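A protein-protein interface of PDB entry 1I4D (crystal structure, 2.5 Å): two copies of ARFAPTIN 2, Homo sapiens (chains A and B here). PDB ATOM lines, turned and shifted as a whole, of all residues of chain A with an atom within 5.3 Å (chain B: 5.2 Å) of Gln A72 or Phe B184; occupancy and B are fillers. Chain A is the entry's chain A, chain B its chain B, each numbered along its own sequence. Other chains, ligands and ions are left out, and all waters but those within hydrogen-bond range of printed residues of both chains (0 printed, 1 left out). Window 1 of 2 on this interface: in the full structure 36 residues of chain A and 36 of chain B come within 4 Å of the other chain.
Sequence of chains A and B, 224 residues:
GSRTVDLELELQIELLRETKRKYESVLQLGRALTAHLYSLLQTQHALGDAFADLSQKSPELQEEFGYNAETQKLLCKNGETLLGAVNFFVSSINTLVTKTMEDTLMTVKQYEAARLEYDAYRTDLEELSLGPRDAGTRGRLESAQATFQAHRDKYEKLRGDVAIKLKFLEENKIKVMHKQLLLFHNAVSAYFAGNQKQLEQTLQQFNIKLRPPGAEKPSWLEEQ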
ATOM      1  N   GLN A  44      11.120 -16.544 -20.126  1.00  0.00           N
ATOM      2  CA  GLN A  44      11.562 -17.928 -20.079  1.00  0.00           C
ATOM      3  C   GLN A  44      12.324 -18.252 -21.357  1.00  0.00           C
ATOM      4  O   GLN A  44      13.369 -18.888 -21.318  1.00  0.00           O
ATOM      5  CB  GLN A  44      10.364 -18.863 -19.913  1.00  0.00           C
ATOM      6  CG  GLN A  44       9.594 -18.625 -18.627  1.00  0.00           C
ATOM      7  CD  GLN A  44       8.413 -19.553 -18.466  1.00  0.00           C
ATOM      8  OE1 GLN A  44       7.517 -19.586 -19.312  1.00  0.00           O
ATOM      9  NE2 GLN A  44       8.402 -20.317 -17.372  1.00  0.00           N
ATOM     10  N   HIS A  45      11.815 -17.800 -22.493  1.00  0.00           N
ATOM     11  CA  HIS A  45      12.503 -18.045 -23.754  1.00  0.00           C
ATOM     12  C   HIS A  45      13.914 -17.462 -23.698  1.00  0.00           C
ATOM     13  O   HIS A  45      14.884 -18.089 -24.128  1.00  0.00           O
ATOM     14  CB  HIS A  45      11.778 -17.381 -24.925  1.00  0.00           C
ATOM     15  CG  HIS A  45      12.502 -17.529 -26.225  1.00  0.00           C
ATOM     16  ND1 HIS A  45      12.316 -18.609 -27.061  1.00  0.00           N
ATOM     17  CD2 HIS A  45      13.499 -16.796 -26.775  1.00  0.00           C
ATOM     18  CE1 HIS A  45      13.170 -18.540 -28.067  1.00  0.00           C
ATOM     19  NE2 HIS A  45      13.901 -17.449 -27.915  1.00  0.00           N
ATOM     20  N   LEU A  47      15.744 -16.530 -20.949  1.00  0.00           N
ATOM     21  CA  LEU A  47      16.506 -17.213 -19.916  1.00  0.00           C
ATOM     22  C   LEU A  47      16.917 -18.595 -20.410  1.00  0.00           C
ATOM     23  O   LEU A  47      17.943 -19.138 -20.008  1.00  0.00           O
ATOM     24  CB  LEU A  47      15.654 -17.318 -18.645  1.00  0.00           C
ATOM     25  CG  LEU A  47      16.429 -17.319 -17.325  1.00  0.00           C
ATOM     26  CD1 LEU A  47      17.456 -16.190 -17.296  1.00  0.00           C
ATOM     27  CD2 LEU A  47      15.427 -17.164 -16.192  1.00  0.00           C
ATOM     28  N   GLY A  48      16.118 -19.162 -21.297  1.00  0.00           N
ATOM     29  CA  GLY A  48      16.461 -20.469 -21.815  1.00  0.00           C
ATOM     30  C   GLY A  48      17.711 -20.371 -22.665  1.00  0.00           C
ATOM     31  O   GLY A  48      18.687 -21.092 -22.457  1.00  0.00           O
ATOM     32  N   PHE A  51      20.829 -19.557 -20.345  1.00  0.00           N
ATOM     33  CA  PHE A  51      21.357 -20.714 -19.632  1.00  0.00           C
ATOM     34  C   PHE A  51      22.033 -21.649 -20.632  1.00  0.00           C
ATOM     35  O   PHE A  51      23.116 -22.185 -20.377  1.00  0.00           O
ATOM     36  CB  PHE A  51      20.227 -21.448 -18.916  1.00  0.00           C
ATOM     37  CG  PHE A  51      19.750 -20.761 -17.673  1.00  0.00           C
ATOM     38  CD1 PHE A  51      18.499 -21.054 -17.143  1.00  0.00           C
ATOM     39  CD2 PHE A  51      20.562 -19.849 -17.005  1.00  0.00           C
ATOM     40  CE1 PHE A  51      18.063 -20.456 -15.967  1.00  0.00           C
ATOM     41  CE2 PHE A  51      20.129 -19.242 -15.819  1.00  0.00           C
ATOM     42  CZ  PHE A  51      18.877 -19.551 -15.305  1.00  0.00           C
ATOM     43  N   ASN A  68      18.811 -26.243 -16.349  1.00  0.00           N
ATOM     44  CA  ASN A  68      17.863 -25.141 -16.279  1.00  0.00           C
ATOM     45  C   ASN A  68      17.425 -24.641 -17.638  1.00  0.00           C
ATOM     46  O   ASN A  68      16.261 -24.281 -17.833  1.00  0.00           O
ATOM     47  CB  ASN A  68      18.465 -23.994 -15.470  1.00  0.00           C
ATOM     48  CG  ASN A  68      18.281 -24.176 -13.975  1.00  0.00           C
ATOM     49  OD1 ASN A  68      17.206 -23.917 -13.438  1.00  0.00           O
ATOM     50  ND2 ASN A  68      19.327 -24.633 -13.299  1.00  0.00           N
ATOM     51  N   ALA A  69      18.361 -24.613 -18.578  1.00  0.00           N
ATOM     52  CA  ALA A  69      18.041 -24.161 -19.917  1.00  0.00           C
ATOM     53  C   ALA A  69      16.832 -24.934 -20.429  1.00  0.00           C
ATOM     54  O   ALA A  69      15.822 -24.335 -20.788  1.00  0.00           O
ATOM     55  CB  ALA A  69      19.228 -24.365 -20.843  1.00  0.00           C
ATOM     56  N   GLU A  70      16.919 -26.260 -20.442  1.00  0.00           N
ATOM     57  CA  GLU A  70      15.810 -27.065 -20.935  1.00  0.00           C
ATOM     58  C   GLU A  70      14.488 -26.828 -20.242  1.00  0.00           C
ATOM     59  O   GLU A  70      13.489 -26.567 -20.910  1.00  0.00           O
ATOM     60  CB  GLU A  70      16.132 -28.554 -20.861  1.00  0.00           C
ATOM     61  CG  GLU A  70      17.364 -28.957 -21.634  1.00  0.00           C
ATOM     62  CD  GLU A  70      17.388 -28.393 -23.049  1.00  0.00           C
ATOM     63  OE1 GLU A  70      17.409 -27.142 -23.190  1.00  0.00           O
ATOM     64  OE2 GLU A  70      17.386 -29.199 -24.015  1.00  0.00           O
ATOM     65  N   THR A  71      14.455 -26.911 -18.916  1.00  0.00           N
ATOM     66  CA  THR A  71      13.181 -26.719 -18.223  1.00  0.00           C
ATOM     67  C   THR A  71      12.571 -25.379 -18.625  1.00  0.00           C
ATOM     68  O   THR A  71      11.356 -25.261 -18.825  1.00  0.00           O
ATOM     69  CB  THR A  71      13.329 -26.768 -16.689  1.00  0.00           C
ATOM     70  OG1 THR A  71      13.814 -25.506 -16.222  1.00  0.00           O
ATOM     71  CG2 THR A  71      14.301 -27.876 -16.278  1.00  0.00           C
ATOM     72  N   GLN A  72      13.423 -24.368 -18.752  1.00  0.00           N
ATOM     73  CA  GLN A  72      12.963 -23.050 -19.148  1.00  0.00           C
ATOM     74  C   GLN A  72      12.512 -23.088 -20.608  1.00  0.00           C
ATOM     75  O   GLN A  72      11.528 -22.448 -20.966  1.00  0.00           O
ATOM     76  CB  GLN A  72      14.078 -22.031 -18.954  1.00  0.00           C
ATOM     77  CG  GLN A  72      13.688 -20.875 -18.060  1.00  0.00           C
ATOM     78  CD  GLN A  72      12.947 -21.331 -16.825  1.00  0.00           C
ATOM     79  OE1 GLN A  72      13.489 -22.044 -15.973  1.00  0.00           O
ATOM     80  NE2 GLN A  72      11.685 -20.928 -16.724  1.00  0.00           N
ATOM     81  N   LYS A  73      13.224 -23.844 -21.448  1.00  0.00           N
ATOM     82  CA  LYS A  73      12.855 -23.961 -22.861  1.00  0.00           C
ATOM     83  C   LYS A  73      11.544 -24.685 -22.978  1.00  0.00           C
ATOM     84  O   LYS A  73      10.771 -24.443 -23.901  1.00  0.00           O
ATOM     85  CB  LYS A  73      13.919 -24.717 -23.667  1.00  0.00           C
ATOM     86  CG  LYS A  73      15.174 -23.900 -23.950  1.00  0.00           C
ATOM     87  CD  LYS A  73      16.154 -24.628 -24.855  1.00  0.00           C
ATOM     88  CE  LYS A  73      17.320 -23.715 -25.227  1.00  0.00           C
ATOM     89  NZ  LYS A  73      18.175 -24.291 -26.310  1.00  0.00           N
ATOM     90  N   LEU A  74      11.292 -25.577 -22.031  1.00  0.00           N
ATOM     91  CA  LEU A  74      10.047 -26.326 -22.032  1.00  0.00           C
ATOM     92  C   LEU A  74       8.915 -25.469 -21.472  1.00  0.00           C
ATOM     93  O   LEU A  74       7.878 -25.317 -22.111  1.00  0.00           O
ATOM     94  CB  LEU A  74      10.188 -27.603 -21.212  1.00  0.00           C
ATOM     95  CG  LEU A  74       8.855 -28.322 -21.000  1.00  0.00           C
ATOM     96  CD1 LEU A  74       8.261 -28.743 -22.345  1.00  0.00           C
ATOM     97  CD2 LEU A  74       9.071 -29.514 -20.093  1.00  0.00           C
ATOM     98  N   LEU A  75       9.106 -24.906 -20.284  1.00  0.00           N
ATOM     99  CA  LEU A  75       8.078 -24.053 -19.698  1.00  0.00           C
ATOM    100  C   LEU A  75       7.605 -22.963 -20.661  1.00  0.00           C
ATOM    101  O   LEU A  75       6.516 -22.417 -20.502  1.00  0.00           O
ATOM    102  CB  LEU A  75       8.599 -23.395 -18.428  1.00  0.00           C
ATOM    103  CG  LEU A  75       8.129 -24.003 -17.110  1.00  0.00           C
ATOM    104  CD1 LEU A  75       8.608 -25.450 -16.992  1.00  0.00           C
ATOM    105  CD2 LEU A  75       8.656 -23.146 -15.965  1.00  0.00           C
ATOM    106  N   CYS A  76       8.433 -22.632 -21.645  1.00  0.00           N
ATOM    107  CA  CYS A  76       8.076 -21.621 -22.626  1.00  0.00           C
ATOM    108  C   CYS A  76       6.999 -22.170 -23.567  1.00  0.00           C
ATOM    109  O   CYS A  76       5.996 -21.505 -23.828  1.00  0.00           O
ATOM    110  CB  CYS A  76       9.310 -21.215 -23.431  1.00  0.00           C
ATOM    111  SG  CYS A  76       9.102 -19.798 -24.557  1.00  0.00           S
ATOM    112  N   LEU B  33      11.818 -12.132 -14.215  1.00  0.00           N
ATOM    113  CA  LEU B  33      11.078 -13.287 -13.729  1.00  0.00           C
ATOM    114  C   LEU B  33      10.388 -12.991 -12.397  1.00  0.00           C
ATOM    115  O   LEU B  33       9.230 -13.356 -12.180  1.00  0.00           O
ATOM    116  CB  LEU B  33      12.012 -14.491 -13.607  1.00  0.00           C
ATOM    117  CG  LEU B  33      11.287 -15.801 -13.323  1.00  0.00           C
ATOM    118  CD1 LEU B  33      10.137 -15.952 -14.278  1.00  0.00           C
ATOM    119  CD2 LEU B  33      12.239 -16.960 -13.450  1.00  0.00           C
ATOM    120  N   VAL B  86      13.111 -17.613  -6.359  1.00  0.00           N
ATOM    121  CA  VAL B  86      13.657 -16.776  -7.427  1.00  0.00           C
ATOM    122  C   VAL B  86      14.323 -15.502  -6.886  1.00  0.00           C
ATOM    123  O   VAL B  86      15.413 -15.127  -7.329  1.00  0.00           O
ATOM    124  CB  VAL B  86      12.550 -16.369  -8.432  1.00  0.00           C
ATOM    125  CG1 VAL B  86      13.173 -15.745  -9.691  1.00  0.00           C
ATOM    126  CG2 VAL B  86      11.687 -17.576  -8.771  1.00  0.00           C
ATOM    127  N   PHE B  89      17.695 -16.400  -5.575  1.00  0.00           N
ATOM    128  CA  PHE B  89      18.559 -16.688  -6.700  1.00  0.00           C
ATOM    129  C   PHE B  89      19.049 -15.369  -7.297  1.00  0.00           C
ATOM    130  O   PHE B  89      20.255 -15.128  -7.425  1.00  0.00           O
ATOM    131  CB  PHE B  89      17.739 -17.479  -7.703  1.00  0.00           C
ATOM    132  CG  PHE B  89      18.411 -17.697  -9.002  1.00  0.00           C
ATOM    133  CD1 PHE B  89      19.467 -18.585  -9.108  1.00  0.00           C
ATOM    134  CD2 PHE B  89      17.952 -17.052 -10.143  1.00  0.00           C
ATOM    135  CE1 PHE B  89      20.059 -18.841 -10.339  1.00  0.00           C
ATOM    136  CE2 PHE B  89      18.531 -17.295 -11.380  1.00  0.00           C
ATOM    137  CZ  PHE B  89      19.588 -18.194 -11.482  1.00  0.00           C
ATOM    138  N   LYS B 179      25.355 -24.062  -6.489  1.00  0.00           N
ATOM    139  CA  LYS B 179      24.323 -24.059  -5.467  1.00  0.00           C
ATOM    140  C   LYS B 179      23.096 -23.287  -5.953  1.00  0.00           C
ATOM    141  O   LYS B 179      21.975 -23.804  -5.942  1.00  0.00           O
ATOM    142  CB  LYS B 179      24.849 -23.409  -4.187  1.00  0.00           C
ATOM    143  CG  LYS B 179      23.859 -23.434  -3.025  1.00  0.00           C
ATOM    144  CD  LYS B 179      24.309 -22.583  -1.830  1.00  0.00           C
ATOM    145  CE  LYS B 179      23.278 -22.655  -0.686  1.00  0.00           C
ATOM    146  NZ  LYS B 179      23.363 -21.538   0.320  1.00  0.00           N
ATOM    147  N   GLN B 180      23.304 -22.044  -6.383  1.00  0.00           N
ATOM    148  CA  GLN B 180      22.193 -21.227  -6.846  1.00  0.00           C
ATOM    149  C   GLN B 180      21.384 -21.877  -7.948  1.00  0.00           C
ATOM    150  O   GLN B 180      20.176 -22.077  -7.783  1.00  0.00           O
ATOM    151  CB  GLN B 180      22.678 -19.847  -7.290  1.00  0.00           C
ATOM    152  CG  GLN B 180      22.919 -18.892  -6.115  1.00  0.00           C
ATOM    153  CD  GLN B 180      21.939 -19.125  -4.969  1.00  0.00           C
ATOM    154  OE1 GLN B 180      20.719 -19.006  -5.132  1.00  0.00           O
ATOM    155  NE2 GLN B 180      22.468 -19.475  -3.810  1.00  0.00           N
ATOM    156  N   LEU B 181      22.038 -22.211  -9.059  1.00  0.00           N
ATOM    157  CA  LEU B 181      21.358 -22.855 -10.181  1.00  0.00           C
ATOM    158  C   LEU B 181      20.515 -24.015  -9.688  1.00  0.00           C
ATOM    159  O   LEU B 181      19.314 -24.080  -9.938  1.00  0.00           O
ATOM    160  CB  LEU B 181      22.378 -23.356 -11.195  1.00  0.00           C
ATOM    161  CG  LEU B 181      22.418 -22.667 -12.565  1.00  0.00           C
ATOM    162  CD1 LEU B 181      22.225 -21.167 -12.422  1.00  0.00           C
ATOM    163  CD2 LEU B 181      23.756 -22.962 -13.225  1.00  0.00           C
ATOM    164  N   LEU B 182      21.151 -24.931  -8.973  1.00  0.00           N
ATOM    165  CA  LEU B 182      20.457 -26.087  -8.430  1.00  0.00           C
ATOM    166  C   LEU B 182      19.275 -25.703  -7.547  1.00  0.00           C
ATOM    167  O   LEU B 182      18.162 -26.207  -7.738  1.00  0.00           O
ATOM    168  CB  LEU B 182      21.430 -26.957  -7.640  1.00  0.00           C
ATOM    169  CG  LEU B 182      21.699 -28.294  -8.331  1.00  0.00           C
ATOM    170  CD1 LEU B 182      22.346 -28.039  -9.703  1.00  0.00           C
ATOM    171  CD2 LEU B 182      22.579 -29.169  -7.444  1.00  0.00           C
ATOM    172  N   LEU B 183      19.507 -24.828  -6.571  1.00  0.00           N
ATOM    173  CA  LEU B 183      18.413 -24.414  -5.709  1.00  0.00           C
ATOM    174  C   LEU B 183      17.292 -23.922  -6.603  1.00  0.00           C
ATOM    175  O   LEU B 183      16.148 -24.361  -6.488  1.00  0.00           O
ATOM    176  CB  LEU B 183      18.844 -23.294  -4.763  1.00  0.00           C
ATOM    177  CG  LEU B 183      19.624 -23.783  -3.546  1.00  0.00           C
ATOM    178  CD1 LEU B 183      20.047 -22.604  -2.701  1.00  0.00           C
ATOM    179  CD2 LEU B 183      18.764 -24.765  -2.751  1.00  0.00           C
ATOM    180  N   PHE B 184      17.641 -23.015  -7.509  1.00  0.00           N
ATOM    181  CA  PHE B 184      16.677 -22.449  -8.440  1.00  0.00           C
ATOM    182  C   PHE B 184      15.813 -23.521  -9.089  1.00  0.00           C
ATOM    183  O   PHE B 184      14.585 -23.486  -9.015  1.00  0.00           O
ATOM    184  CB  PHE B 184      17.414 -21.678  -9.528  1.00  0.00           C
ATOM    185  CG  PHE B 184      16.513 -21.103 -10.560  1.00  0.00           C
ATOM    186  CD1 PHE B 184      15.661 -20.053 -10.243  1.00  0.00           C
ATOM    187  CD2 PHE B 184      16.489 -21.634 -11.848  1.00  0.00           C
ATOM    188  CE1 PHE B 184      14.793 -19.534 -11.194  1.00  0.00           C
ATOM    189  CE2 PHE B 184      15.625 -21.129 -12.811  1.00  0.00           C
ATOM    190  CZ  PHE B 184      14.773 -20.075 -12.485  1.00  0.00           C
ATOM    191  N   HIS B 185      16.483 -24.473  -9.725  1.00  0.00           N
ATOM    192  CA  HIS B 185      15.840 -25.574 -10.416  1.00  0.00           C
ATOM    193  C   HIS B 185      14.976 -26.454  -9.526  1.00  0.00           C
ATOM    194  O   HIS B 185      13.987 -27.026  -9.982  1.00  0.00           O
ATOM    195  CB  HIS B 185      16.892 -26.439 -11.077  1.00  0.00           C
ATOM    196  CG  HIS B 185      16.333 -27.671 -11.700  1.00  0.00           C
ATOM    197  ND1 HIS B 185      15.585 -27.642 -12.857  1.00  0.00           N
ATOM    198  CD2 HIS B 185      16.349 -28.959 -11.289  1.00  0.00           C
ATOM    199  CE1 HIS B 185      15.162 -28.862 -13.133  1.00  0.00           C
ATOM    200  NE2 HIS B 185      15.611 -29.681 -12.196  1.00  0.00           N
ATOM    201  N   ASN B 186      15.356 -26.604  -8.265  1.00  0.00           N
ATOM    202  CA  ASN B 186      14.545 -27.411  -7.366  1.00  0.00           C
ATOM    203  C   ASN B 186      13.268 -26.657  -7.045  1.00  0.00           C
ATOM    204  O   ASN B 186      12.193 -27.248  -6.962  1.00  0.00           O
ATOM    205  CB  ASN B 186      15.301 -27.700  -6.082  1.00  0.00           C
ATOM    206  CG  ASN B 186      16.491 -28.572  -6.316  1.00  0.00           C
ATOM    207  OD1 ASN B 186      16.362 -29.705  -6.775  1.00  0.00           O
ATOM    208  ND2 ASN B 186      17.669 -28.051  -6.018  1.00  0.00           N
ATOM    209  N   ALA B 187      13.392 -25.346  -6.865  1.00  0.00           N
ATOM    210  CA  ALA B 187      12.234 -24.524  -6.561  1.00  0.00           C
ATOM    211  C   ALA B 187      11.201 -24.677  -7.670  1.00  0.00           C
ATOM    212  O   ALA B 187      10.011 -24.837  -7.405  1.00  0.00           O
ATOM    213  CB  ALA B 187      12.649 -23.068  -6.428  1.00  0.00           C
ATOM    214  N   VAL B 188      11.658 -24.643  -8.916  1.00  0.00           N
ATOM    215  CA  VAL B 188      10.745 -24.774 -10.036  1.00  0.00           C
ATOM    216  C   VAL B 188      10.080 -26.140 -10.018  1.00  0.00           C
ATOM    217  O   VAL B 188       8.868 -26.248 -10.154  1.00  0.00           O
ATOM    218  CB  VAL B 188      11.482 -24.573 -11.383  1.00  0.00           C
ATOM    219  CG1 VAL B 188      10.512 -24.691 -12.550  1.00  0.00           C
ATOM    220  CG2 VAL B 188      12.150 -23.205 -11.406  1.00  0.00           C
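The backbone carbonyl oxygen of Leu B181 lies within hydrogen-bond range of the side-chain amide nitrogen of Asn A68 (3.4 Å).
The side-chain amide nitrogen of Gln A72 lies close to the side-chain amide nitrogen of Gln A44.
The backbone carbonyl oxygen (O) of Asn A68 is in hydrogen-bond range of the side-chain hydroxyl (OG1) of Thr A71.
The side-chain amide oxygen (OE1) of Gln A72 lies within hydrogen-bond range of the side-chain hydroxyl (OG1) of Thr A71, 3.5 Å away.
Among the printed residues, pairs that only touch across the chains: Asn A68 with Phe B184 (2.9 Å), Thr A71 with His B185 (3.4 Å), Asn A68 with His B185 (3.5 Å) and Gln A72 with Phe B184 (3.9 Å).
Of chain B, only Phe B184 (3.9 Å) comes within 4 Å of Gln A72.
Leu A75 touches none of the printed residues of chain B.
Of the printed residues of chain A, Leu B181 touches Asn A68.
Of the printed residues of chain A, Phe B184 touches Asn A68 (2.9 Å) and Gln A72 (3.9 Å).
Of the printed residues of chain A, His B185 touches Asn A68 (3.5 Å) and Thr A71 (3.4 Å).
The nearest residue of chain B that does not touch Gln A72 is Val B188 (4.9 Å).
The nearest residue of chain A that does not touch Phe B184 is Phe A51 (4.04 Å).
Among the printed residues, 5 pairs touch across the chains.
Among the printed residues, no Asp or Glu carboxylate lies within 4 Å of a Lys or Arg side-chain nitrogen of the other chain.
No position is printed for both chains.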
